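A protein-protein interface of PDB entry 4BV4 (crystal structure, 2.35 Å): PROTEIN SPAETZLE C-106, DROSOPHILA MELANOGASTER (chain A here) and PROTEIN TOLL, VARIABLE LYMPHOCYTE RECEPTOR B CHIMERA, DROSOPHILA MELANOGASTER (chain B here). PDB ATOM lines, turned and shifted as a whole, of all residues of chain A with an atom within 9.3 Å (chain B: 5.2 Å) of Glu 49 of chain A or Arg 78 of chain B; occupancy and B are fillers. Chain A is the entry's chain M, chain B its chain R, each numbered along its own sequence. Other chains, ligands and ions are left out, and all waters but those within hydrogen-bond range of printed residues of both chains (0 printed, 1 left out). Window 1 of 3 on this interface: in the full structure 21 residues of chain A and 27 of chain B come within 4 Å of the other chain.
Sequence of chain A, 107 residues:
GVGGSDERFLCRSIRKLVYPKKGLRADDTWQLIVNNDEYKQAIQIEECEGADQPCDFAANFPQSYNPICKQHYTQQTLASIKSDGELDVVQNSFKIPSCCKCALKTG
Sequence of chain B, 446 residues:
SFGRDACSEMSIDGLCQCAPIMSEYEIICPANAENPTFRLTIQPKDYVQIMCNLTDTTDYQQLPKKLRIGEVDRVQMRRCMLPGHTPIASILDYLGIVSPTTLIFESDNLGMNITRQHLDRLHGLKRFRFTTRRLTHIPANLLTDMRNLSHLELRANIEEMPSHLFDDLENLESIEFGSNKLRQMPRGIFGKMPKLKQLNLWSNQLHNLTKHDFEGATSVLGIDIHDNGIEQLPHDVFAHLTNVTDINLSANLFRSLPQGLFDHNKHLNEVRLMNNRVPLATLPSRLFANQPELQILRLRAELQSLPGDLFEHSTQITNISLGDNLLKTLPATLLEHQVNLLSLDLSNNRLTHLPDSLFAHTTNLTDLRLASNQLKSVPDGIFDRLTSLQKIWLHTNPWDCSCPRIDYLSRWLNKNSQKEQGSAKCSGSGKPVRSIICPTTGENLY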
ATOM      1  N   GLY A   1     -12.913  13.429  30.694  1.00  0.00           N
ATOM      2  CA  GLY A   1     -12.442  14.190  29.552  1.00  0.00           C
ATOM      3  C   GLY A   1     -10.937  14.351  29.509  1.00  0.00           C
ATOM      4  O   GLY A   1     -10.451  15.439  29.189  1.00  0.00           O
ATOM      5  N   VAL A   2     -10.181  13.271  29.810  1.00  0.00           N
ATOM      6  CA  VAL A   2      -8.711  13.295  29.778  1.00  0.00           C
ATOM      7  C   VAL A   2      -8.216  13.058  28.335  1.00  0.00           C
ATOM      8  O   VAL A   2      -7.471  13.886  27.805  1.00  0.00           O
ATOM      9  CB  VAL A   2      -8.070  12.290  30.771  1.00  0.00           C
ATOM     10  CG1 VAL A   2      -6.544  12.374  30.740  1.00  0.00           C
ATOM     11  CG2 VAL A   2      -8.588  12.516  32.187  1.00  0.00           C
ATOM     12  N   GLY A   3      -8.628  11.934  27.738  1.00  0.00           N
ATOM     13  CA  GLY A   3      -8.254  11.531  26.386  1.00  0.00           C
ATOM     14  C   GLY A   3      -6.968  10.727  26.324  1.00  0.00           C
ATOM     15  O   GLY A   3      -6.229  10.651  27.312  1.00  0.00           O
ATOM     16  N   PHE A   9      -8.937  17.017  20.536  1.00  0.00           N
ATOM     17  CA  PHE A   9     -10.368  17.120  20.271  1.00  0.00           C
ATOM     18  C   PHE A   9     -10.776  18.541  19.956  1.00  0.00           C
ATOM     19  O   PHE A   9     -10.138  19.471  20.420  1.00  0.00           O
ATOM     20  CB  PHE A   9     -11.168  16.599  21.475  1.00  0.00           C
ATOM     21  CG  PHE A   9     -10.922  15.143  21.790  1.00  0.00           C
ATOM     22  CD1 PHE A   9     -11.553  14.142  21.062  1.00  0.00           C
ATOM     23  CD2 PHE A   9     -10.059  14.773  22.819  1.00  0.00           C
ATOM     24  CE1 PHE A   9     -11.307  12.796  21.343  1.00  0.00           C
ATOM     25  CE2 PHE A   9      -9.816  13.427  23.100  1.00  0.00           C
ATOM     26  CZ  PHE A   9     -10.450  12.449  22.367  1.00  0.00           C
ATOM     27  N   LEU A  10     -11.837  18.704  19.167  1.00  0.00           N
ATOM     28  CA  LEU A  10     -12.363  19.999  18.760  1.00  0.00           C
ATOM     29  C   LEU A  10     -13.046  20.684  19.935  1.00  0.00           C
ATOM     30  O   LEU A  10     -13.063  21.917  20.005  1.00  0.00           O
ATOM     31  CB  LEU A  10     -13.344  19.830  17.582  1.00  0.00           C
ATOM     32  CG  LEU A  10     -12.711  19.721  16.198  1.00  0.00           C
ATOM     33  CD1 LEU A  10     -12.619  18.288  15.749  1.00  0.00           C
ATOM     34  CD2 LEU A  10     -13.506  20.499  15.183  1.00  0.00           C
ATOM     35  N   CYS A  11     -13.616  19.883  20.849  1.00  0.00           N
ATOM     36  CA  CYS A  11     -14.274  20.370  22.065  1.00  0.00           C
ATOM     37  C   CYS A  11     -13.783  19.565  23.264  1.00  0.00           C
ATOM     38  O   CYS A  11     -13.710  18.335  23.188  1.00  0.00           O
ATOM     39  CB  CYS A  11     -15.791  20.286  21.949  1.00  0.00           C
ATOM     40  SG  CYS A  11     -16.496  21.244  20.588  1.00  0.00           S
ATOM     41  N   ARG A  12     -13.481  20.244  24.369  1.00  0.00           N
ATOM     42  CA  ARG A  12     -13.045  19.632  25.627  1.00  0.00           C
ATOM     43  C   ARG A  12     -14.189  19.586  26.620  1.00  0.00           C
ATOM     44  O   ARG A  12     -14.882  20.592  26.839  1.00  0.00           O
ATOM     45  CB  ARG A  12     -11.859  20.393  26.270  1.00  0.00           C
ATOM     46  CG  ARG A  12     -10.559  20.385  25.482  1.00  0.00           C
ATOM     47  CD  ARG A  12      -9.920  19.010  25.369  1.00  0.00           C
ATOM     48  NE  ARG A  12      -8.945  18.994  24.275  1.00  0.00           N
ATOM     49  CZ  ARG A  12      -8.087  18.009  24.029  1.00  0.00           C
ATOM     50  NH1 ARG A  12      -8.070  16.923  24.796  1.00  0.00           N
ATOM     51  NH2 ARG A  12      -7.229  18.110  23.027  1.00  0.00           N
ATOM     52  N   SER A  13     -14.347  18.426  27.256  1.00  0.00           N
ATOM     53  CA  SER A  13     -15.347  18.220  28.294  1.00  0.00           C
ATOM     54  C   SER A  13     -14.683  18.043  29.665  1.00  0.00           C
ATOM     55  O   SER A  13     -13.484  17.747  29.747  1.00  0.00           O
ATOM     56  CB  SER A  13     -16.225  17.017  27.960  1.00  0.00           C
ATOM     57  OG  SER A  13     -15.435  15.858  27.757  1.00  0.00           O
ATOM     58  N   ILE A  14     -15.468  18.238  30.732  1.00  0.00           N
ATOM     59  CA  ILE A  14     -15.046  18.040  32.124  1.00  0.00           C
ATOM     60  C   ILE A  14     -15.890  16.884  32.682  1.00  0.00           C
ATOM     61  O   ILE A  14     -17.120  16.923  32.568  1.00  0.00           O
ATOM     62  CB  ILE A  14     -15.150  19.352  32.967  1.00  0.00           C
ATOM     63  CG1 ILE A  14     -14.185  20.420  32.423  1.00  0.00           C
ATOM     64  CG2 ILE A  14     -14.882  19.093  34.465  1.00  0.00           C
ATOM     65  CD1 ILE A  14     -14.534  21.822  32.805  1.00  0.00           C
ATOM     66  N   ARG A  15     -15.228  15.838  33.228  1.00  0.00           N
ATOM     67  CA  ARG A  15     -15.918  14.674  33.787  1.00  0.00           C
ATOM     68  C   ARG A  15     -16.322  14.940  35.233  1.00  0.00           C
ATOM     69  O   ARG A  15     -15.569  15.592  35.970  1.00  0.00           O
ATOM     70  CB  ARG A  15     -15.060  13.401  33.680  1.00  0.00           C
ATOM     71  CG  ARG A  15     -13.801  13.347  34.563  1.00  0.00           C
ATOM     72  CD  ARG A  15     -12.755  12.340  34.096  1.00  0.00           C
ATOM     73  NE  ARG A  15     -13.223  10.950  34.152  1.00  0.00           N
ATOM     74  CZ  ARG A  15     -13.285  10.136  33.102  1.00  0.00           C
ATOM     75  NH1 ARG A  15     -12.907  10.557  31.900  1.00  0.00           N
ATOM     76  NH2 ARG A  15     -13.720   8.892  33.245  1.00  0.00           N
ATOM     77  N   GLU A  46     -20.427  14.064  31.281  1.00  0.00           N
ATOM     78  CA  GLU A  46     -19.401  14.804  30.548  1.00  0.00           C
ATOM     79  C   GLU A  46     -20.007  16.113  30.086  1.00  0.00           C
ATOM     80  O   GLU A  46     -20.957  16.109  29.302  1.00  0.00           O
ATOM     81  CB  GLU A  46     -18.811  13.999  29.388  1.00  0.00           C
ATOM     82  CG  GLU A  46     -17.991  12.802  29.839  1.00  0.00           C
ATOM     83  CD  GLU A  46     -16.589  13.056  30.371  1.00  0.00           C
ATOM     84  OE1 GLU A  46     -16.056  14.174  30.173  1.00  0.00           O
ATOM     85  OE2 GLU A  46     -15.995  12.099  30.923  1.00  0.00           O
ATOM     86  N   GLU A  47     -19.520  17.226  30.652  1.00  0.00           N
ATOM     87  CA  GLU A  47     -20.035  18.556  30.338  1.00  0.00           C
ATOM     88  C   GLU A  47     -19.018  19.408  29.591  1.00  0.00           C
ATOM     89  O   GLU A  47     -17.820  19.279  29.842  1.00  0.00           O
ATOM     90  CB  GLU A  47     -20.481  19.287  31.615  1.00  0.00           C
ATOM     91  CG  GLU A  47     -21.730  18.685  32.227  1.00  0.00           C
ATOM     92  CD  GLU A  47     -22.717  19.685  32.794  1.00  0.00           C
ATOM     93  OE1 GLU A  47     -22.527  20.114  33.957  1.00  0.00           O
ATOM     94  OE2 GLU A  47     -23.702  20.011  32.087  1.00  0.00           O
ATOM     95  N   CYS A  48     -19.506  20.299  28.694  1.00  0.00           N
ATOM     96  CA  CYS A  48     -18.688  21.271  27.964  1.00  0.00           C
ATOM     97  C   CYS A  48     -18.003  22.205  28.953  1.00  0.00           C
ATOM     98  O   CYS A  48     -18.659  22.699  29.868  1.00  0.00           O
ATOM     99  CB  CYS A  48     -19.541  22.066  26.976  1.00  0.00           C
ATOM    100  SG  CYS A  48     -20.233  21.089  25.626  1.00  0.00           S
ATOM    101  N   GLU A  49     -16.694  22.448  28.754  1.00  0.00           N
ATOM    102  CA  GLU A  49     -15.832  23.371  29.515  1.00  0.00           C
ATOM    103  C   GLU A  49     -16.299  24.802  29.155  1.00  0.00           C
ATOM    104  O   GLU A  49     -15.628  25.519  28.401  1.00  0.00           O
ATOM    105  CB  GLU A  49     -14.356  23.091  29.130  1.00  0.00           C
ATOM    106  CG  GLU A  49     -13.279  23.797  29.934  1.00  0.00           C
ATOM    107  CD  GLU A  49     -11.888  23.189  29.853  1.00  0.00           C
ATOM    108  OE1 GLU A  49     -11.523  22.661  28.776  1.00  0.00           O
ATOM    109  OE2 GLU A  49     -11.146  23.269  30.860  1.00  0.00           O
ATOM    110  N   GLY A  50     -17.502  25.153  29.623  1.00  0.00           N
ATOM    111  CA  GLY A  50     -18.179  26.401  29.284  1.00  0.00           C
ATOM    112  C   GLY A  50     -18.920  26.262  27.961  1.00  0.00           C
ATOM    113  O   GLY A  50     -18.496  25.488  27.089  1.00  0.00           O
ATOM    114  N   ALA A  51     -20.051  26.986  27.795  1.00  0.00           N
ATOM    115  CA  ALA A  51     -20.860  26.919  26.562  1.00  0.00           C
ATOM    116  C   ALA A  51     -21.442  28.303  26.183  1.00  0.00           C
ATOM    117  O   ALA A  51     -21.728  29.072  27.094  1.00  0.00           O
ATOM    118  CB  ALA A  51     -21.984  25.900  26.730  1.00  0.00           C
ATOM    119  N   ASP A  52     -21.624  28.652  24.875  1.00  0.00           N
ATOM    120  CA  ASP A  52     -21.353  27.874  23.652  1.00  0.00           C
ATOM    121  C   ASP A  52     -20.147  28.476  22.903  1.00  0.00           C
ATOM    122  O   ASP A  52     -20.264  29.471  22.185  1.00  0.00           O
ATOM    123  CB  ASP A  52     -22.603  27.818  22.755  1.00  0.00           C
ATOM    124  CG  ASP A  52     -23.773  27.083  23.382  1.00  0.00           C
ATOM    125  OD1 ASP A  52     -23.733  25.829  23.426  1.00  0.00           O
ATOM    126  OD2 ASP A  52     -24.742  27.758  23.807  1.00  0.00           O
ATOM    127  N   GLN A  53     -18.981  27.863  23.119  1.00  0.00           N
ATOM    128  CA  GLN A  53     -17.674  28.275  22.613  1.00  0.00           C
ATOM    129  C   GLN A  53     -17.400  27.757  21.208  1.00  0.00           C
ATOM    130  O   GLN A  53     -17.861  26.660  20.874  1.00  0.00           O
ATOM    131  CB  GLN A  53     -16.559  27.726  23.546  1.00  0.00           C
ATOM    132  CG  GLN A  53     -16.842  27.746  25.050  1.00  0.00           C
ATOM    133  CD  GLN A  53     -16.909  29.139  25.628  1.00  0.00           C
ATOM    134  OE1 GLN A  53     -15.943  29.916  25.577  1.00  0.00           O
ATOM    135  NE2 GLN A  53     -18.051  29.468  26.218  1.00  0.00           N
ATOM    136  N   PRO A  54     -16.576  28.461  20.394  1.00  0.00           N
ATOM    137  CA  PRO A  54     -16.187  27.889  19.100  1.00  0.00           C
ATOM    138  C   PRO A  54     -15.295  26.663  19.285  1.00  0.00           C
ATOM    139  O   PRO A  54     -14.559  26.579  20.275  1.00  0.00           O
ATOM    140  CB  PRO A  54     -15.404  29.023  18.419  1.00  0.00           C
ATOM    141  CG  PRO A  54     -15.648  30.253  19.244  1.00  0.00           C
ATOM    142  CD  PRO A  54     -15.886  29.747  20.630  1.00  0.00           C
ATOM    143  N   CYS A  69     -19.152  24.318  19.928  1.00  0.00           N
ATOM    144  CA  CYS A  69     -19.178  23.206  20.882  1.00  0.00           C
ATOM    145  C   CYS A  69     -20.558  23.107  21.488  1.00  0.00           C
ATOM    146  O   CYS A  69     -21.069  24.070  22.058  1.00  0.00           O
ATOM    147  CB  CYS A  69     -18.105  23.388  21.948  1.00  0.00           C
ATOM    148  SG  CYS A  69     -16.425  23.134  21.337  1.00  0.00           S
ATOM    149  N   LYS A  70     -21.176  21.959  21.321  1.00  0.00           N
ATOM    150  CA  LYS A  70     -22.537  21.726  21.768  1.00  0.00           C
ATOM    151  C   LYS A  70     -22.630  20.553  22.731  1.00  0.00           C
ATOM    152  O   LYS A  70     -22.041  19.494  22.491  1.00  0.00           O
ATOM    153  CB  LYS A  70     -23.436  21.488  20.544  1.00  0.00           C
ATOM    154  CG  LYS A  70     -24.651  22.405  20.471  1.00  0.00           C
ATOM    155  CD  LYS A  70     -24.308  23.852  20.103  1.00  0.00           C
ATOM    156  CE  LYS A  70     -25.411  24.790  20.534  1.00  0.00           C
ATOM    157  NZ  LYS A  70     -24.998  26.212  20.434  1.00  0.00           N
ATOM    158  N   GLN A  71     -23.393  20.757  23.819  1.00  0.00           N
ATOM    159  CA  GLN A  71     -23.666  19.747  24.826  1.00  0.00           C
ATOM    160  C   GLN A  71     -24.663  18.676  24.298  1.00  0.00           C
ATOM    161  O   GLN A  71     -25.776  18.997  23.857  1.00  0.00           O
ATOM    162  CB  GLN A  71     -24.199  20.404  26.102  1.00  0.00           C
ATOM    163  CG  GLN A  71     -24.466  19.431  27.258  1.00  0.00           C
ATOM    164  CD  GLN A  71     -23.193  18.883  27.841  1.00  0.00           C
ATOM    165  OE1 GLN A  71     -22.396  19.613  28.446  1.00  0.00           O
ATOM    166  NE2 GLN A  71     -22.968  17.593  27.644  1.00  0.00           N
ATOM    167  N   CYS A  99     -21.688  14.216  26.477  1.00  0.00           N
ATOM    168  CA  CYS A  99     -20.683  14.608  25.499  1.00  0.00           C
ATOM    169  C   CYS A  99     -20.756  16.068  25.182  1.00  0.00           C
ATOM    170  O   CYS A  99     -21.808  16.700  25.248  1.00  0.00           O
ATOM    171  CB  CYS A  99     -20.839  13.799  24.213  1.00  0.00           C
ATOM    172  SG  CYS A  99     -19.561  12.545  23.959  1.00  0.00           S
ATOM    173  N   CYS A 100     -19.619  16.576  24.751  1.00  0.00           N
ATOM    174  CA  CYS A 100     -19.469  17.871  24.156  1.00  0.00           C
ATOM    175  C   CYS A 100     -19.006  17.613  22.740  1.00  0.00           C
ATOM    176  O   CYS A 100     -17.984  16.965  22.557  1.00  0.00           O
ATOM    177  CB  CYS A 100     -18.498  18.747  24.931  1.00  0.00           C
ATOM    178  SG  CYS A 100     -18.620  20.497  24.504  1.00  0.00           S
ATOM    179  N   LYS A 101     -19.781  18.041  21.741  1.00  0.00           N
ATOM    180  CA  LYS A 101     -19.460  17.773  20.339  1.00  0.00           C
ATOM    181  C   LYS A 101     -19.389  19.038  19.525  1.00  0.00           C
ATOM    182  O   LYS A 101     -20.047  20.015  19.868  1.00  0.00           O
ATOM    183  CB  LYS A 101     -20.509  16.841  19.699  1.00  0.00           C
ATOM    184  CG  LYS A 101     -20.385  15.386  20.055  1.00  0.00           C
ATOM    185  CD  LYS A 101     -20.940  14.451  18.946  1.00  0.00           C
ATOM    186  CE  LYS A 101     -22.382  14.633  18.499  1.00  0.00           C
ATOM    187  NZ  LYS A 101     -23.322  14.837  19.635  1.00  0.00           N
ATOM    188  N   GLN B  49      -4.003  13.092  35.117  1.00  0.00           N
ATOM    189  CA  GLN B  49      -4.613  14.400  34.922  1.00  0.00           C
ATOM    190  C   GLN B  49      -4.966  14.992  36.282  1.00  0.00           C
ATOM    191  O   GLN B  49      -5.589  14.325  37.113  1.00  0.00           O
ATOM    192  CB  GLN B  49      -5.845  14.364  34.000  1.00  0.00           C
ATOM    193  CG  GLN B  49      -6.345  15.775  33.690  1.00  0.00           C
ATOM    194  CD  GLN B  49      -7.737  15.852  33.131  1.00  0.00           C
ATOM    195  OE1 GLN B  49      -7.928  16.031  31.930  1.00  0.00           O
ATOM    196  NE2 GLN B  49      -8.737  15.849  33.997  1.00  0.00           N
ATOM    197  N   ILE B  50      -4.545  16.243  36.502  1.00  0.00           N
ATOM    198  CA  ILE B  50      -4.816  17.005  37.710  1.00  0.00           C
ATOM    199  C   ILE B  50      -5.720  18.168  37.312  1.00  0.00           C
ATOM    200  O   ILE B  50      -5.325  18.971  36.465  1.00  0.00           O
ATOM    201  CB  ILE B  50      -3.493  17.481  38.385  1.00  0.00           C
ATOM    202  CG1 ILE B  50      -2.467  16.330  38.500  1.00  0.00           C
ATOM    203  CG2 ILE B  50      -3.764  18.120  39.761  1.00  0.00           C
ATOM    204  CD1 ILE B  50      -1.020  16.728  38.358  1.00  0.00           C
ATOM    205  N   MET B  51      -6.952  18.222  37.857  1.00  0.00           N
ATOM    206  CA  MET B  51      -7.837  19.350  37.588  1.00  0.00           C
ATOM    207  C   MET B  51      -8.083  20.121  38.869  1.00  0.00           C
ATOM    208  O   MET B  51      -8.722  19.627  39.809  1.00  0.00           O
ATOM    209  CB  MET B  51      -9.147  19.001  36.899  1.00  0.00           C
ATOM    210  CG  MET B  51      -9.634  20.176  36.070  1.00  0.00           C
ATOM    211  SD  MET B  51     -11.298  20.094  35.384  1.00  0.00           S
ATOM    212  CE  MET B  51     -11.031  19.017  34.026  1.00  0.00           C
ATOM    213  N   CYS B  52      -7.550  21.342  38.892  1.00  0.00           N
ATOM    214  CA  CYS B  52      -7.613  22.238  40.031  1.00  0.00           C
ATOM    215  C   CYS B  52      -8.816  23.168  39.947  1.00  0.00           C
ATOM    216  O   CYS B  52      -9.263  23.526  38.855  1.00  0.00           O
ATOM    217  CB  CYS B  52      -6.321  23.047  40.144  1.00  0.00           C
ATOM    218  SG  CYS B  52      -4.793  22.071  40.070  1.00  0.00           S
ATOM    219  N   GLN B  76      -0.944  15.902  32.674  1.00  0.00           N
ATOM    220  CA  GLN B  76      -1.872  16.917  32.195  1.00  0.00           C
ATOM    221  C   GLN B  76      -2.459  17.705  33.373  1.00  0.00           C
ATOM    222  O   GLN B  76      -3.063  17.125  34.272  1.00  0.00           O
ATOM    223  CB  GLN B  76      -2.976  16.255  31.360  1.00  0.00           C
ATOM    224  CG  GLN B  76      -3.881  17.229  30.622  1.00  0.00           C
ATOM    225  CD  GLN B  76      -4.702  16.488  29.606  1.00  0.00           C
ATOM    226  OE1 GLN B  76      -4.181  15.992  28.607  1.00  0.00           O
ATOM    227  NE2 GLN B  76      -5.996  16.352  29.862  1.00  0.00           N
ATOM    228  N   MET B  77      -2.258  19.027  33.370  1.00  0.00           N
ATOM    229  CA  MET B  77      -2.763  19.904  34.423  1.00  0.00           C
ATOM    230  C   MET B  77      -3.736  20.882  33.828  1.00  0.00           C
ATOM    231  O   MET B  77      -3.371  21.651  32.943  1.00  0.00           O
ATOM    232  CB  MET B  77      -1.625  20.621  35.142  1.00  0.00           C
ATOM    233  CG  MET B  77      -1.191  19.926  36.393  1.00  0.00           C
ATOM    234  SD  MET B  77       0.272  20.678  37.151  1.00  0.00           S
ATOM    235  CE  MET B  77       1.491  20.126  36.012  1.00  0.00           C
ATOM    236  N   ARG B  78      -4.988  20.815  34.274  1.00  0.00           N
ATOM    237  CA  ARG B  78      -6.045  21.678  33.765  1.00  0.00           C
ATOM    238  C   ARG B  78      -6.546  22.589  34.838  1.00  0.00           C
ATOM    239  O   ARG B  78      -6.808  22.132  35.954  1.00  0.00           O
ATOM    240  CB  ARG B  78      -7.216  20.867  33.194  1.00  0.00           C
ATOM    241  CG  ARG B  78      -6.961  20.296  31.830  1.00  0.00           C
ATOM    242  CD  ARG B  78      -7.975  19.230  31.485  1.00  0.00           C
ATOM    243  NE  ARG B  78      -9.270  19.777  31.078  1.00  0.00           N
ATOM    244  CZ  ARG B  78     -10.311  19.038  30.716  1.00  0.00           C
ATOM    245  NH1 ARG B  78     -10.232  17.714  30.740  1.00  0.00           N
ATOM    246  NH2 ARG B  78     -11.453  19.612  30.373  1.00  0.00           N
ATOM    247  N   ARG B  79      -6.673  23.889  34.503  1.00  0.00           N
ATOM    248  CA  ARG B  79      -7.199  24.965  35.357  1.00  0.00           C
ATOM    249  C   ARG B  79      -6.345  25.222  36.611  1.00  0.00           C
ATOM    250  O   ARG B  79      -6.848  25.818  37.571  1.00  0.00           O
ATOM    251  CB  ARG B  79      -8.665  24.658  35.768  1.00  0.00           C
ATOM    252  CG  ARG B  79      -9.552  24.232  34.604  1.00  0.00           C
ATOM    253  CD  ARG B  79     -11.005  24.250  34.972  1.00  0.00           C
ATOM    254  NE  ARG B  79     -11.828  24.578  33.810  1.00  0.00           N
ATOM    255  CZ  ARG B  79     -13.096  24.962  33.880  1.00  0.00           C
ATOM    256  NH1 ARG B  79     -13.700  25.073  35.057  1.00  0.00           N
ATOM    257  NH2 ARG B  79     -13.773  25.243  32.774  1.00  0.00           N
ATOM    258  N   CYS B  80      -5.056  24.819  36.606  1.00  0.00           N
ATOM    259  CA  CYS B  80      -4.182  24.987  37.776  1.00  0.00           C
ATOM    260  C   CYS B  80      -3.354  26.251  37.717  1.00  0.00           C
ATOM    261  O   CYS B  80      -2.845  26.611  36.676  1.00  0.00           O
ATOM    262  CB  CYS B  80      -3.287  23.769  37.974  1.00  0.00           C
ATOM    263  SG  CYS B  80      -4.186  22.206  38.127  1.00  0.00           S
ATOM    264  N   GLU B 106      -2.787  23.515  30.916  1.00  0.00           N
ATOM    265  CA  GLU B 106      -3.879  24.277  30.291  1.00  0.00           C
ATOM    266  C   GLU B 106      -4.660  25.024  31.355  1.00  0.00           C
ATOM    267  O   GLU B 106      -5.271  24.384  32.202  1.00  0.00           O
ATOM    268  CB  GLU B 106      -4.798  23.343  29.488  1.00  0.00           C
ATOM    269  CG  GLU B 106      -4.106  22.708  28.292  1.00  0.00           C
ATOM    270  CD  GLU B 106      -4.756  21.467  27.705  1.00  0.00           C
ATOM    271  OE1 GLU B 106      -5.174  20.584  28.493  1.00  0.00           O
ATOM    272  OE2 GLU B 106      -4.749  21.330  26.458  1.00  0.00           O
ATOM    273  N   SER B 107      -4.608  26.367  31.367  1.00  0.00           N
ATOM    274  CA  SER B 107      -5.273  27.126  32.439  1.00  0.00           C
ATOM    275  C   SER B 107      -5.544  28.571  32.072  1.00  0.00           C
ATOM    276  O   SER B 107      -4.746  29.175  31.372  1.00  0.00           O
ATOM    277  CB  SER B 107      -4.422  27.100  33.706  1.00  0.00           C
ATOM    278  OG  SER B 107      -5.071  27.779  34.769  1.00  0.00           O
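Of chain B, only Arg 78 (3.4 Å) and Arg 79 (3.2 Å) come within 4 Å of Glu 49 of chain A. Arg 78 of chain B touches four residues of chain A. Of the printed residues of chain B, Ile 14 of chain A touches Met 51 (3.8 Å), Arg 78 (3.5 Å) and Arg 79 (3.5 Å). Of the printed residues of chain A, Gln 76 of chain B touches Val 2 (3.5 Å). Lys 70 of chain A touches none of the printed residues of chain B. The nearest printed residue of chain B that does not touch Ile 14 of chain A is Gln 49 of chain B (6.9 Å).
The backbone carbonyl oxygen (O) of Gly 1 of chain A is in hydrogen-bond range of the guanidinium group (NH1) of Arg 78 of chain B (2.8 Å). NH2 of Arg 78 of chain B is in hydrogen-bond range of O of Ser 13 of chain A (2.8 Å). The side-chain carboxylate (OE1) of Glu 49 of chain A is in salt-bridge range of the guanidinium group (NH2) of Arg 78 of chain B, 3.4 Å away. OE2 of Glu 49 of chain A lies within salt-bridge range of NE of Arg 79 of chain B (3.3 Å).
Gly 1 of chain A touches Gln 49 of chain B (O to OE1, 3.8 Å). Gln 49 of chain B touches Val 2 of chain A (OE1 to CA, 3.6 Å). O of Val 2 of chain A touches NE2 of Gln 76 of chain B, at 3.5 Å. Ile 14 of chain A touches Met 51 of chain B (CG1 to CE, 3.8 Å). Ile 14 of chain A touches Arg 78 of chain B. Ile 14 of chain A touches Arg 79 of chain B (CD1 to NH2, 3.5 Å).
The backbone NH of Ile 14 of chain A lies within hydrogen-bond range of the backbone carbonyl oxygen of Glu 47 of chain A (2.7 Å). The side-chain amide oxygen (OE1) of Gln 49 of chain B is in hydrogen-bond range of the side-chain amide nitrogen (NE2) of Gln 76 of chain B, 2.8 Å away. N of Cys 52 of chain B lies within hydrogen-bond range of O of Arg 78 of chain B (3.1 Å). The side-chain sulfur (SG) of Cys 69 of chain A is disulfide-bonded to the side-chain sulfur (SG) of Cys 11 of chain A, at 2.0 Å. The side-chain sulfur (SG) of Cys 48 of chain A forms a disulfide with the side-chain sulfur (SG) of Cys 100 of chain A (2.1 Å). SG of Cys 52 of chain B is disulfide-bonded to SG of Cys 80 of chain B (2.0 Å).
Of the 25 printed residues of chain A, 5 touch a printed residue of chain B. Of the 11 printed residues of chain B, 5 touch a printed residue of chain A. Hydrophobic or aromatic side chains of chain B within 4 Å of the printed part of chain A: Met 51. Among the printed residues, Asp or Glu carboxylates within 4 Å of a Lys or Arg side-chain nitrogen of the other chain: Glu 49 of chain A with Arg 78 of chain B (3.4 Å) and Glu 49 of chain A with Arg 79 of chain B (3.3 Å).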
